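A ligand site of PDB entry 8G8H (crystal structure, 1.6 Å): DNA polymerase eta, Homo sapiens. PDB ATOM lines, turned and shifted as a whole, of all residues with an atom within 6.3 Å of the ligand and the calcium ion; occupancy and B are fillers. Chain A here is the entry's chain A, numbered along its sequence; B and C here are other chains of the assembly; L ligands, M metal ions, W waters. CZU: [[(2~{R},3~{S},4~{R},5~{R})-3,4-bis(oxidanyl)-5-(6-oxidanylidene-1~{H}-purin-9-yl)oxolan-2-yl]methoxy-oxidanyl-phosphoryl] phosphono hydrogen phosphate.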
ATOM      1  N   ASP A  13      24.941  -5.354 -16.947  1.00  0.00           N
ATOM      2  CA  ASP A  13      24.924  -6.251 -15.793  1.00  0.00           C
ATOM      3  C   ASP A  13      25.650  -7.542 -16.182  1.00  0.00           C
ATOM      4  O   ASP A  13      25.206  -8.253 -17.085  1.00  0.00           O
ATOM      5  CB  ASP A  13      23.467  -6.540 -15.381  1.00  0.00           C
ATOM      6  CG  ASP A  13      23.338  -7.332 -14.113  1.00  0.00           C
ATOM      7  OD1 ASP A  13      24.005  -8.345 -13.974  1.00  0.00           O
ATOM      8  OD2 ASP A  13      22.488  -6.975 -13.275  1.00  0.00           O
ATOM      9  N   MET A  14      26.760  -7.852 -15.503  1.00  0.00           N
ATOM     10  CA  MET A  14      27.496  -9.060 -15.847  1.00  0.00           C
ATOM     11  C   MET A  14      26.644 -10.291 -15.509  1.00  0.00           C
ATOM     12  O   MET A  14      26.036 -10.341 -14.436  1.00  0.00           O
ATOM     13  CB  MET A  14      28.817  -9.111 -15.086  1.00  0.00           C
ATOM     14  CG  MET A  14      29.736  -7.940 -15.372  1.00  0.00           C
ATOM     15  SD  MET A  14      29.947  -7.425 -17.062  1.00  0.00           S
ATOM     16  CE  MET A  14      30.939  -8.781 -17.677  1.00  0.00           C
ATOM     17  N   ASP A  15      26.562 -11.252 -16.420  1.00  0.00           N
ATOM     18  CA  ASP A  15      25.804 -12.470 -16.149  1.00  0.00           C
ATOM     19  C   ASP A  15      26.566 -13.312 -15.128  1.00  0.00           C
ATOM     20  O   ASP A  15      27.774 -13.482 -15.247  1.00  0.00           O
ATOM     21  CB  ASP A  15      25.629 -13.270 -17.428  1.00  0.00           C
ATOM     22  CG  ASP A  15      24.824 -12.522 -18.482  1.00  0.00           C
ATOM     23  OD1 ASP A  15      23.946 -11.746 -18.101  1.00  0.00           O
ATOM     24  OD2 ASP A  15      25.117 -12.705 -19.681  1.00  0.00           O
ATOM     25  N   CYS A  16      25.836 -13.893 -14.164  1.00  0.00           N
ATOM     26  CA  CYS A  16      26.418 -14.708 -13.077  1.00  0.00           C
ATOM     27  C   CYS A  16      27.904 -14.426 -12.841  1.00  0.00           C
ATOM     28  O   CYS A  16      28.750 -15.297 -13.085  1.00  0.00           O
ATOM     29  CB  CYS A  16      26.207 -16.211 -13.352  1.00  0.00           C
ATOM     30  SG  CYS A  16      26.652 -16.874 -14.981  1.00  0.00           S
ATOM     31  N   PHE A  17      28.218 -13.216 -12.376  1.00  0.00           N
ATOM     32  CA  PHE A  17      29.563 -12.676 -12.556  1.00  0.00           C
ATOM     33  C   PHE A  17      30.621 -13.538 -11.889  1.00  0.00           C
ATOM     34  O   PHE A  17      31.629 -13.877 -12.521  1.00  0.00           O
ATOM     35  CB  PHE A  17      29.637 -11.255 -12.041  1.00  0.00           C
ATOM     36  CG  PHE A  17      30.965 -10.583 -12.322  1.00  0.00           C
ATOM     37  CD1 PHE A  17      31.574 -10.719 -13.550  1.00  0.00           C
ATOM     38  CD2 PHE A  17      31.613  -9.883 -11.316  1.00  0.00           C
ATOM     39  CE1 PHE A  17      32.827 -10.126 -13.806  1.00  0.00           C
ATOM     40  CE2 PHE A  17      32.864  -9.288 -11.559  1.00  0.00           C
ATOM     41  CZ  PHE A  17      33.457  -9.412 -12.798  1.00  0.00           C
ATOM     42  N   PHE A  18      30.448 -13.881 -10.605  1.00  0.00           N
ATOM     43  CA  PHE A  18      31.508 -14.618  -9.911  1.00  0.00           C
ATOM     44  C   PHE A  18      31.773 -15.967 -10.587  1.00  0.00           C
ATOM     45  O   PHE A  18      32.919 -16.449 -10.635  1.00  0.00           O
ATOM     46  CB  PHE A  18      31.163 -14.832  -8.440  1.00  0.00           C
ATOM     47  CG  PHE A  18      31.263 -13.585  -7.574  1.00  0.00           C
ATOM     48  CD1 PHE A  18      31.355 -12.318  -8.121  1.00  0.00           C
ATOM     49  CD2 PHE A  18      31.286 -13.719  -6.194  1.00  0.00           C
ATOM     50  CE1 PHE A  18      31.436 -11.185  -7.294  1.00  0.00           C
ATOM     51  CE2 PHE A  18      31.385 -12.600  -5.369  1.00  0.00           C
ATOM     52  CZ  PHE A  18      31.467 -11.338  -5.924  1.00  0.00           C
ATOM     53  N   VAL A  19      30.707 -16.607 -11.070  1.00  0.00           N
ATOM     54  CA  VAL A  19      30.838 -17.858 -11.809  1.00  0.00           C
ATOM     55  C   VAL A  19      31.658 -17.653 -13.080  1.00  0.00           C
ATOM     56  O   VAL A  19      32.557 -18.455 -13.387  1.00  0.00           O
ATOM     57  CB  VAL A  19      29.445 -18.442 -12.132  1.00  0.00           C
ATOM     58  CG1 VAL A  19      29.533 -19.506 -13.221  1.00  0.00           C
ATOM     59  CG2 VAL A  19      28.850 -19.032 -10.866  1.00  0.00           C
ATOM     60  N   ILE A  48      26.857 -18.023  -3.508  1.00  0.00           N
ATOM     61  CA  ILE A  48      26.763 -16.601  -3.818  1.00  0.00           C
ATOM     62  C   ILE A  48      26.600 -16.304  -5.296  1.00  0.00           C
ATOM     63  O   ILE A  48      26.228 -15.176  -5.641  1.00  0.00           O
ATOM     64  CB  ILE A  48      27.941 -15.799  -3.222  1.00  0.00           C
ATOM     65  CG1 ILE A  48      29.287 -16.227  -3.786  1.00  0.00           C
ATOM     66  CG2 ILE A  48      27.955 -15.929  -1.684  1.00  0.00           C
ATOM     67  CD1 ILE A  48      30.433 -15.689  -2.956  1.00  0.00           C
ATOM     68  N   ALA A  49      26.825 -17.258  -6.185  1.00  0.00           N
ATOM     69  CA  ALA A  49      26.574 -17.055  -7.603  1.00  0.00           C
ATOM     70  C   ALA A  49      26.336 -18.409  -8.246  1.00  0.00           C
ATOM     71  O   ALA A  49      26.907 -19.406  -7.820  1.00  0.00           O
ATOM     72  CB  ALA A  49      27.738 -16.320  -8.281  1.00  0.00           C
ATOM     73  N   VAL A  50      25.468 -18.441  -9.264  1.00  0.00           N
ATOM     74  CA  VAL A  50      24.969 -19.694  -9.847  1.00  0.00           C
ATOM     75  C   VAL A  50      24.971 -19.589 -11.378  1.00  0.00           C
ATOM     76  O   VAL A  50      24.381 -18.659 -11.934  1.00  0.00           O
ATOM     77  CB  VAL A  50      23.544 -20.016  -9.358  1.00  0.00           C
ATOM     78  CG1 VAL A  50      23.137 -21.382  -9.838  1.00  0.00           C
ATOM     79  CG2 VAL A  50      23.433 -19.928  -7.861  1.00  0.00           C
ATOM     80  N   TYR A  52      23.900 -20.433 -15.239  1.00  0.00           N
ATOM     81  CA  TYR A  52      22.569 -20.637 -15.785  1.00  0.00           C
ATOM     82  C   TYR A  52      22.239 -22.119 -15.945  1.00  0.00           C
ATOM     83  O   TYR A  52      21.073 -22.506 -15.771  1.00  0.00           O
ATOM     84  CB  TYR A  52      22.424 -19.829 -17.096  1.00  0.00           C
ATOM     85  CG  TYR A  52      22.149 -18.368 -16.764  1.00  0.00           C
ATOM     86  CD1 TYR A  52      23.170 -17.499 -16.406  1.00  0.00           C
ATOM     87  CD2 TYR A  52      20.846 -17.882 -16.751  1.00  0.00           C
ATOM     88  CE1 TYR A  52      22.903 -16.170 -16.062  1.00  0.00           C
ATOM     89  CE2 TYR A  52      20.567 -16.568 -16.407  1.00  0.00           C
ATOM     90  CZ  TYR A  52      21.597 -15.707 -16.067  1.00  0.00           C
ATOM     91  OH  TYR A  52      21.308 -14.399 -15.731  1.00  0.00           O
ATOM     92  N   ARG A  55      20.979 -23.043 -12.583  1.00  0.00           N
ATOM     93  CA  ARG A  55      19.669 -22.448 -12.322  1.00  0.00           C
ATOM     94  C   ARG A  55      18.538 -23.295 -12.886  1.00  0.00           C
ATOM     95  O   ARG A  55      17.428 -23.287 -12.332  1.00  0.00           O
ATOM     96  CB  ARG A  55      19.615 -21.035 -12.900  1.00  0.00           C
ATOM     97  CG  ARG A  55      20.594 -20.090 -12.227  1.00  0.00           C
ATOM     98  CD  ARG A  55      20.491 -18.703 -12.823  1.00  0.00           C
ATOM     99  NE  ARG A  55      21.655 -17.895 -12.486  1.00  0.00           N
ATOM    100  CZ  ARG A  55      21.686 -16.577 -12.543  1.00  0.00           C
ATOM    101  NH1 ARG A  55      20.625 -15.871 -12.932  1.00  0.00           N
ATOM    102  NH2 ARG A  55      22.792 -15.936 -12.184  1.00  0.00           N
ATOM    103  N   ARG A  61      21.100 -18.351  -5.480  1.00  0.00           N
ATOM    104  CA  ARG A  61      21.838 -17.641  -4.445  1.00  0.00           C
ATOM    105  C   ARG A  61      21.181 -17.826  -3.099  1.00  0.00           C
ATOM    106  O   ARG A  61      19.960 -17.974  -2.994  1.00  0.00           O
ATOM    107  CB  ARG A  61      21.901 -16.150  -4.777  1.00  0.00           C
ATOM    108  CG  ARG A  61      23.080 -15.426  -4.196  1.00  0.00           C
ATOM    109  CD  ARG A  61      23.054 -13.975  -4.624  1.00  0.00           C
ATOM    110  NE  ARG A  61      21.682 -13.476  -4.654  1.00  0.00           N
ATOM    111  CZ  ARG A  61      21.141 -12.852  -5.683  1.00  0.00           C
ATOM    112  NH1 ARG A  61      21.807 -12.660  -6.810  1.00  0.00           N
ATOM    113  NH2 ARG A  61      19.886 -12.409  -5.580  1.00  0.00           N
ATOM    114  N   LEU A  89      37.060 -10.978  -1.549  1.00  0.00           N
ATOM    115  CA  LEU A  89      36.438 -10.787  -2.852  1.00  0.00           C
ATOM    116  C   LEU A  89      37.388 -10.150  -3.863  1.00  0.00           C
ATOM    117  O   LEU A  89      36.931  -9.783  -4.960  1.00  0.00           O
ATOM    118  CB  LEU A  89      35.182  -9.912  -2.679  1.00  0.00           C
ATOM    119  CG  LEU A  89      34.043 -10.583  -1.898  1.00  0.00           C
ATOM    120  CD1 LEU A  89      32.775  -9.709  -1.895  1.00  0.00           C
ATOM    121  CD2 LEU A  89      33.756 -11.980  -2.403  1.00  0.00           C
ATOM    122  N   SER A 113      27.456  -1.400  -8.659  1.00  0.00           N
ATOM    123  CA  SER A 113      27.765  -2.550  -7.810  1.00  0.00           C
ATOM    124  C   SER A 113      29.043  -3.164  -8.365  1.00  0.00           C
ATOM    125  O   SER A 113      29.645  -2.636  -9.305  1.00  0.00           O
ATOM    126  CB  SER A 113      26.612  -3.559  -7.785  1.00  0.00           C
ATOM    127  OG  SER A 113      26.597  -4.313  -9.001  1.00  0.00           O
ATOM    128  N   ILE A 114      29.449  -4.305  -7.808  1.00  0.00           N
ATOM    129  CA  ILE A 114      30.656  -4.962  -8.294  1.00  0.00           C
ATOM    130  C   ILE A 114      30.486  -5.374  -9.741  1.00  0.00           C
ATOM    131  O   ILE A 114      31.468  -5.511 -10.481  1.00  0.00           O
ATOM    132  CB  ILE A 114      30.996  -6.158  -7.395  1.00  0.00           C
ATOM    133  CG1 ILE A 114      32.339  -6.747  -7.776  1.00  0.00           C
ATOM    134  CG2 ILE A 114      29.909  -7.223  -7.479  1.00  0.00           C
ATOM    135  CD1 ILE A 114      33.091  -7.385  -6.613  1.00  0.00           C
ATOM    136  N   ASP A 115      29.240  -5.563 -10.209  1.00  0.00           N
ATOM    137  CA  ASP A 115      29.096  -6.102 -11.547  1.00  0.00           C
ATOM    138  C   ASP A 115      28.052  -5.374 -12.404  1.00  0.00           C
ATOM    139  O   ASP A 115      27.656  -5.917 -13.441  1.00  0.00           O
ATOM    140  CB  ASP A 115      28.789  -7.585 -11.463  1.00  0.00           C
ATOM    141  CG  ASP A 115      27.333  -7.878 -11.298  1.00  0.00           C
ATOM    142  OD1 ASP A 115      26.666  -7.124 -10.541  1.00  0.00           O
ATOM    143  OD2 ASP A 115      26.864  -8.866 -11.904  1.00  0.00           O
ATOM    144  N   GLU A 116      27.627  -4.175 -12.034  1.00  0.00           N
ATOM    145  CA  GLU A 116      26.809  -3.396 -12.943  1.00  0.00           C
ATOM    146  C   GLU A 116      27.243  -1.941 -12.950  1.00  0.00           C
ATOM    147  O   GLU A 116      27.848  -1.438 -12.008  1.00  0.00           O
ATOM    148  CB  GLU A 116      25.293  -3.512 -12.691  1.00  0.00           C
ATOM    149  CG  GLU A 116      24.794  -3.793 -11.350  1.00  0.00           C
ATOM    150  CD  GLU A 116      23.297  -4.042 -11.383  1.00  0.00           C
ATOM    151  OE1 GLU A 116      22.563  -3.045 -11.377  1.00  0.00           O
ATOM    152  OE2 GLU A 116      22.839  -5.207 -11.458  1.00  0.00           O
ATOM    153  N   LYS A 224      17.414  -0.556 -16.060  1.00  0.00           N
ATOM    154  CA  LYS A 224      17.581  -1.696 -15.172  1.00  0.00           C
ATOM    155  C   LYS A 224      16.504  -2.742 -15.419  1.00  0.00           C
ATOM    156  O   LYS A 224      16.795  -3.947 -15.489  1.00  0.00           O
ATOM    157  CB  LYS A 224      17.564  -1.205 -13.721  1.00  0.00           C
ATOM    158  CG  LYS A 224      17.553  -2.302 -12.681  1.00  0.00           C
ATOM    159  CD  LYS A 224      18.793  -3.159 -12.758  1.00  0.00           C
ATOM    160  CE  LYS A 224      18.877  -4.039 -11.510  1.00  0.00           C
ATOM    161  NZ  LYS A 224      19.868  -5.139 -11.657  1.00  0.00           N
ATOM    162  N   LYS A 231      17.810 -12.062 -20.285  1.00  0.00           N
ATOM    163  CA  LYS A 231      19.076 -12.536 -19.738  1.00  0.00           C
ATOM    164  C   LYS A 231      19.244 -14.017 -20.069  1.00  0.00           C
ATOM    165  O   LYS A 231      18.263 -14.740 -20.237  1.00  0.00           O
ATOM    166  CB  LYS A 231      19.108 -12.329 -18.217  1.00  0.00           C
ATOM    167  CG  LYS A 231      19.840 -11.057 -17.722  1.00  0.00           C
ATOM    168  CD  LYS A 231      20.241 -11.119 -16.218  1.00  0.00           C
ATOM    169  CE  LYS A 231      21.302 -10.066 -15.844  1.00  0.00           C
ATOM    170  NZ  LYS A 231      22.765 -10.473 -16.064  1.00  0.00           N
ATOM    171  N   PRO A 232      20.465 -14.550 -20.218  1.00  0.00           N
ATOM    172  CA  PRO A 232      21.792 -13.925 -20.257  1.00  0.00           C
ATOM    173  C   PRO A 232      22.249 -13.566 -21.656  1.00  0.00           C
ATOM    174  O   PRO A 232      21.653 -14.016 -22.643  1.00  0.00           O
ATOM    175  CB  PRO A 232      22.689 -15.037 -19.695  1.00  0.00           C
ATOM    176  CG  PRO A 232      22.093 -16.267 -20.292  1.00  0.00           C
ATOM    177  CD  PRO A 232      20.583 -16.018 -20.356  1.00  0.00           C
ATOM    178  P    DT B   3      19.216 -19.146   7.424  1.00  0.00           P
ATOM    179  OP1  DT B   3      18.595 -18.154   8.340  1.00  0.00           O
ATOM    180  OP2  DT B   3      18.521 -20.401   7.055  1.00  0.00           O
ATOM    181  O5'  DT B   3      19.589 -18.394   6.066  1.00  0.00           O
ATOM    182  C5'  DT B   3      20.107 -17.063   6.105  1.00  0.00           C
ATOM    183  C4'  DT B   3      21.593 -17.077   5.814  1.00  0.00           C
ATOM    184  O4'  DT B   3      21.819 -16.921   4.385  1.00  0.00           O
ATOM    185  C3'  DT B   3      22.404 -15.967   6.485  1.00  0.00           C
ATOM    186  O3'  DT B   3      23.715 -16.459   6.700  1.00  0.00           O
ATOM    187  C2'  DT B   3      22.414 -14.924   5.383  1.00  0.00           C
ATOM    188  C1'  DT B   3      22.711 -15.837   4.213  1.00  0.00           C
ATOM    189  N1   DT B   3      22.533 -15.220   2.846  1.00  0.00           N
ATOM    190  C2   DT B   3      23.552 -15.359   1.923  1.00  0.00           C
ATOM    191  O2   DT B   3      24.586 -15.965   2.171  1.00  0.00           O
ATOM    192  N3   DT B   3      23.330 -14.774   0.707  1.00  0.00           N
ATOM    193  C4   DT B   3      22.204 -14.057   0.320  1.00  0.00           C
ATOM    194  O4   DT B   3      22.094 -13.565  -0.807  1.00  0.00           O
ATOM    195  C5   DT B   3      21.157 -13.942   1.331  1.00  0.00           C
ATOM    196  C7   DT B   3      19.889 -13.200   1.024  1.00  0.00           C
ATOM    197  C6   DT B   3      21.371 -14.521   2.529  1.00  0.00           C
ATOM    198  P    DC B   4      24.621 -15.952   7.934  1.00  0.00           P
ATOM    199  OP1  DC B   4      25.097 -17.204   8.582  1.00  0.00           O
ATOM    200  OP2  DC B   4      23.886 -14.944   8.725  1.00  0.00           O
ATOM    201  O5'  DC B   4      25.852 -15.247   7.199  1.00  0.00           O
ATOM    202  C5'  DC B   4      26.478 -15.891   6.078  1.00  0.00           C
ATOM    203  C4'  DC B   4      27.263 -14.905   5.229  1.00  0.00           C
ATOM    204  O4'  DC B   4      26.394 -14.307   4.229  1.00  0.00           O
ATOM    205  C3'  DC B   4      27.881 -13.743   6.003  1.00  0.00           C
ATOM    206  O3'  DC B   4      29.161 -13.476   5.499  1.00  0.00           O
ATOM    207  C2'  DC B   4      26.914 -12.587   5.712  1.00  0.00           C
ATOM    208  C1'  DC B   4      26.519 -12.903   4.282  1.00  0.00           C
ATOM    209  N1   DC B   4      25.216 -12.280   3.860  1.00  0.00           N
ATOM    210  C2   DC B   4      25.087 -11.771   2.573  1.00  0.00           C
ATOM    211  O2   DC B   4      26.055 -11.835   1.816  1.00  0.00           O
ATOM    212  N3   DC B   4      23.911 -11.216   2.193  1.00  0.00           N
ATOM    213  C4   DC B   4      22.886 -11.165   3.045  1.00  0.00           C
ATOM    214  N4   DC B   4      21.746 -10.602   2.626  1.00  0.00           N
ATOM    215  C5   DC B   4      22.995 -11.682   4.374  1.00  0.00           C
ATOM    216  C6   DC B   4      24.169 -12.223   4.736  1.00  0.00           C
ATOM    217  P    DC B   5      30.151 -12.518   6.310  1.00  0.00           P
ATOM    218  OP1  DC B   5      31.505 -12.588   5.730  1.00  0.00           O
ATOM    219  OP2  DC B   5      29.923 -12.709   7.753  1.00  0.00           O
ATOM    220  O5'  DC B   5      29.565 -11.072   6.036  1.00  0.00           O
ATOM    221  C5'  DC B   5      30.435 -10.040   5.754  1.00  0.00           C
ATOM    222  C4'  DC B   5      30.388  -9.681   4.283  1.00  0.00           C
ATOM    223  O4'  DC B   5      29.057  -9.896   3.769  1.00  0.00           O
ATOM    224  C3'  DC B   5      30.707  -8.229   4.031  1.00  0.00           C
ATOM    225  O3'  DC B   5      31.944  -8.097   3.458  1.00  0.00           O
ATOM    226  C2'  DC B   5      29.612  -7.733   3.078  1.00  0.00           C
ATOM    227  C1'  DC B   5      28.846  -8.984   2.712  1.00  0.00           C
ATOM    228  N1   DC B   5      27.433  -8.696   2.635  1.00  0.00           N
ATOM    229  C2   DC B   5      26.895  -8.159   1.448  1.00  0.00           C
ATOM    230  O2   DC B   5      27.639  -7.979   0.475  1.00  0.00           O
ATOM    231  N3   DC B   5      25.586  -7.872   1.410  1.00  0.00           N
ATOM    232  C4   DC B   5      24.819  -8.079   2.479  1.00  0.00           C
ATOM    233  N4   DC B   5      23.526  -7.770   2.382  1.00  0.00           N
ATOM    234  C5   DC B   5      25.341  -8.602   3.690  1.00  0.00           C
ATOM    235  C6   DC B   5      26.646  -8.886   3.719  1.00  0.00           C
ATOM    236  P    DG C   8      19.060  -5.349  -7.441  1.00  0.00           P
ATOM    237  OP1  DG C   8      18.288  -5.242  -8.695  1.00  0.00           O
ATOM    238  OP2  DG C   8      18.740  -6.442  -6.477  1.00  0.00           O
ATOM    239  O5'  DG C   8      20.626  -5.476  -7.762  1.00  0.00           O
ATOM    240  C5'  DG C   8      21.422  -4.323  -8.015  1.00  0.00           C
ATOM    241  C4'  DG C   8      22.889  -4.684  -7.848  1.00  0.00           C
ATOM    242  O4'  DG C   8      23.208  -4.752  -6.445  1.00  0.00           O
ATOM    243  C3'  DG C   8      23.267  -6.050  -8.435  1.00  0.00           C
ATOM    244  O3'  DG C   8      24.561  -5.988  -9.037  1.00  0.00           O
ATOM    245  C2'  DG C   8      23.245  -6.977  -7.219  1.00  0.00           C
ATOM    246  C1'  DG C   8      23.645  -6.042  -6.081  1.00  0.00           C
ATOM    247  N9   DG C   8      23.049  -6.377  -4.790  1.00  0.00           N
ATOM    248  C8   DG C   8      21.728  -6.565  -4.520  1.00  0.00           C
ATOM    249  N7   DG C   8      21.468  -6.832  -3.272  1.00  0.00           N
ATOM    250  C5   DG C   8      22.714  -6.836  -2.679  1.00  0.00           C
ATOM    251  C6   DG C   8      23.075  -7.078  -1.331  1.00  0.00           C
ATOM    252  O6   DG C   8      22.328  -7.345  -0.385  1.00  0.00           O
ATOM    253  N1   DG C   8      24.451  -6.992  -1.149  1.00  0.00           N
ATOM    254  C2   DG C   8      25.353  -6.707  -2.144  1.00  0.00           C
ATOM    255  N2   DG C   8      26.646  -6.648  -1.788  1.00  0.00           N
ATOM    256  N3   DG C   8      25.034  -6.479  -3.402  1.00  0.00           N
ATOM    257  C4   DG C   8      23.697  -6.557  -3.601  1.00  0.00           C
HETATM  258  C2  CZU L   1      25.287 -10.392  -0.758  1.00  0.00           C
HETATM  259  C4  CZU L   1      24.780  -9.983  -3.018  1.00  0.00           C
HETATM  260  C5  CZU L   1      23.488 -10.232  -2.782  1.00  0.00           C
HETATM  261  C6  CZU L   1      23.077 -10.548  -1.544  1.00  0.00           C
HETATM  262  O6  CZU L   1      21.755 -10.789  -1.337  1.00  0.00           O
HETATM  263  C1' CZU L   1      26.291  -9.357  -4.865  1.00  0.00           C
HETATM  264  C2' CZU L   1      27.223 -10.577  -5.020  1.00  0.00           C
HETATM  265  C3' CZU L   1      26.838 -11.011  -6.412  1.00  0.00           C
HETATM  266  C4' CZU L   1      26.895  -9.676  -7.095  1.00  0.00           C
HETATM  267  C5' CZU L   1      26.186  -9.749  -8.450  1.00  0.00           C
HETATM  268  C8  CZU L   1      23.728  -9.739  -4.879  1.00  0.00           C
HETATM  269  N1  CZU L   1      23.951 -10.647  -0.536  1.00  0.00           N
HETATM  270  N3  CZU L   1      25.700 -10.055  -2.037  1.00  0.00           N
HETATM  271  N7  CZU L   1      22.842 -10.077  -3.944  1.00  0.00           N
HETATM  272  N9  CZU L   1      24.930  -9.685  -4.304  1.00  0.00           N
HETATM  273  O1A CZU L   1      23.944  -9.427 -10.442  1.00  0.00           O
HETATM  274  O1B CZU L   1      25.411 -13.714  -9.935  1.00  0.00           O
HETATM  275  O1G CZU L   1      23.088 -13.240 -13.948  1.00  0.00           O
HETATM  276  O2' CZU L   1      28.617 -10.167  -5.058  1.00  0.00           O
HETATM  277  O2A CZU L   1      22.373 -10.140  -8.523  1.00  0.00           O
HETATM  278  O2B CZU L   1      25.676 -11.673 -11.498  1.00  0.00           O
HETATM  279  O2G CZU L   1      21.418 -12.827 -12.093  1.00  0.00           O
HETATM  280  O3' CZU L   1      27.876 -11.882  -6.952  1.00  0.00           O
HETATM  281  O3A CZU L   1      23.866 -11.866  -9.581  1.00  0.00           O
HETATM  282  O3B CZU L   1      23.609 -13.243 -11.646  1.00  0.00           O
HETATM  283  O3G CZU L   1      23.178 -11.092 -12.634  1.00  0.00           O
HETATM  284  O4' CZU L   1      26.072  -8.873  -6.243  1.00  0.00           O
HETATM  285  O5' CZU L   1      24.813 -10.059  -8.158  1.00  0.00           O
HETATM  286  PA  CZU L   1      23.665 -10.286  -9.260  1.00  0.00           P
HETATM  287  PB  CZU L   1      24.776 -12.601 -10.723  1.00  0.00           P
HETATM  288  PG  CZU L   1      22.689 -12.475 -12.775  1.00  0.00           P
HETATM  289 CA    CA M   1      24.937  -9.716 -12.509  1.00  0.00          CA
HETATM  290  O   HOH W   1      20.625 -13.105  -9.832  1.00  0.00           O
HETATM  291  O   HOH W   2      24.546 -13.479  -6.982  1.00  0.00           O
HETATM  292  O   HOH W   3      28.161 -13.088  -9.155  1.00  0.00           O
HETATM  293  O   HOH W   4      24.228 -15.940  -9.647  1.00  0.00           O
HETATM  294  O   HOH W   5      21.048  -8.925 -11.857  1.00  0.00           O
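An oxygen (O1G) of the ligand is in hydrogen-bond range of the side-chain hydroxyl (OH) of Tyr 52 (2.8 Å).
A nitrogen (N1) of the ligand sits at hydrogen-bond distance from N3 of DC 4 of chain B, 2.8 Å away.
N of Cys 16 sits at hydrogen-bond distance from O1G of the ligand, at 2.8 Å.
A nitrogen (N1) of the ligand lies close to O4 of DT 3 of chain B.
The guanidinium group of Arg 55 lies within salt-bridge range of an oxygen (O1G) of the ligand.
NH1 of Arg 61 is in salt-bridge range of O2A of the ligand (3.1 Å).
An oxygen (O2B) of the ligand sits close to the backbone NH of Phe 17 (3.1 Å).
NZ of Lys 231 is in salt-bridge range of O1G of the ligand (3.5 Å).
The side-chain hydroxyl of Ser 113 lies close to the backbone NH of Asp 115.
O of Asp 13 is in hydrogen-bond range of NZ of Lys 231, at 3.5 Å.
OD2 of Asp 13 lies close to OE2 of Glu 116 (2.6 Å).
The side-chain carboxylate (OD2) of Asp 13 lies within salt-bridge range of the side-chain amino group (NZ) of Lys 224, at 3.6 Å.
The side-chain hydroxyl (OH) of Tyr 52 is in hydrogen-bond range of the guanidinium group (NH1) of Arg 55 (3.2 Å).
O3' of DG 8 of chain C is in hydrogen-bond range of OG of Ser 113, at 2.6 Å.
The side-chain amino group of Lys 224 lies within salt-bridge range of OP1 of DG 8 of chain C, 3.4 Å away.
The side-chain amino group of Lys 231 lies within salt-bridge range of the side-chain carboxylate of Asp 15 (2.7 Å).
N3 of DG 8 of chain C lies close to a nitrogen (N9) of the ligand, 3.3 Å away.
Asp 15 touches the ligand.
Phe 18 touches the ligand (CZ to O2', 3.2 Å).
O of Ile 48 touches O3' of the ligand, 3.9 Å away.
Ala 49 touches the ligand (CB to O1B, 3.9 Å).
Ile 114 touches the ligand (CG2 to C4', 3.9 Å).
N3 of DC 5 of chain B touches C2 of the ligand (3.3 Å).
The nearest printed residue that does not touch the ligand is Glu 116 (4.5 Å).
Within 4 Å of the calcium ion: Asp 13, Met 14 and Asp 115.
The calcium ion is bound by OD2 of Asp 115 (2.2 Å).
The calcium ion is bound by OD1 of Asp 13 (2.2 Å).
O3G of the ligand is bound to the calcium ion (2.2 Å).
The calcium ion is bound by the backbone carbonyl oxygen (O) of Met 14 (2.3 Å).
The calcium ion is bound by O1A of the ligand (2.3 Å).
O2B of the ligand is bound to the calcium ion, 2.3 Å away.
Water W1 bridges an oxygen (O2G) of the ligand (2.4 Å) and the guanidinium group (NH1) of Arg 61 (3.3 Å).
Water W3 lies within hydrogen-bond range of an oxygen (O3') of the ligand (2.5 Å), the backbone NH of Phe 18 (2.8 Å) and the backbone NH of Phe 17 (3.2 Å).
Water W4 lies within hydrogen-bond range of an oxygen (O1B) of the ligand (2.5 Å), the backbone NH of Val 50 (2.8 Å) and the guanidinium group of Arg 55 (2.9 Å).
Water W2 lies within hydrogen-bond range of the backbone carbonyl oxygen (O) of Ile 48, the guanidinium group (NH1) of Arg 61 and an oxygen (O1B) of the ligand.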
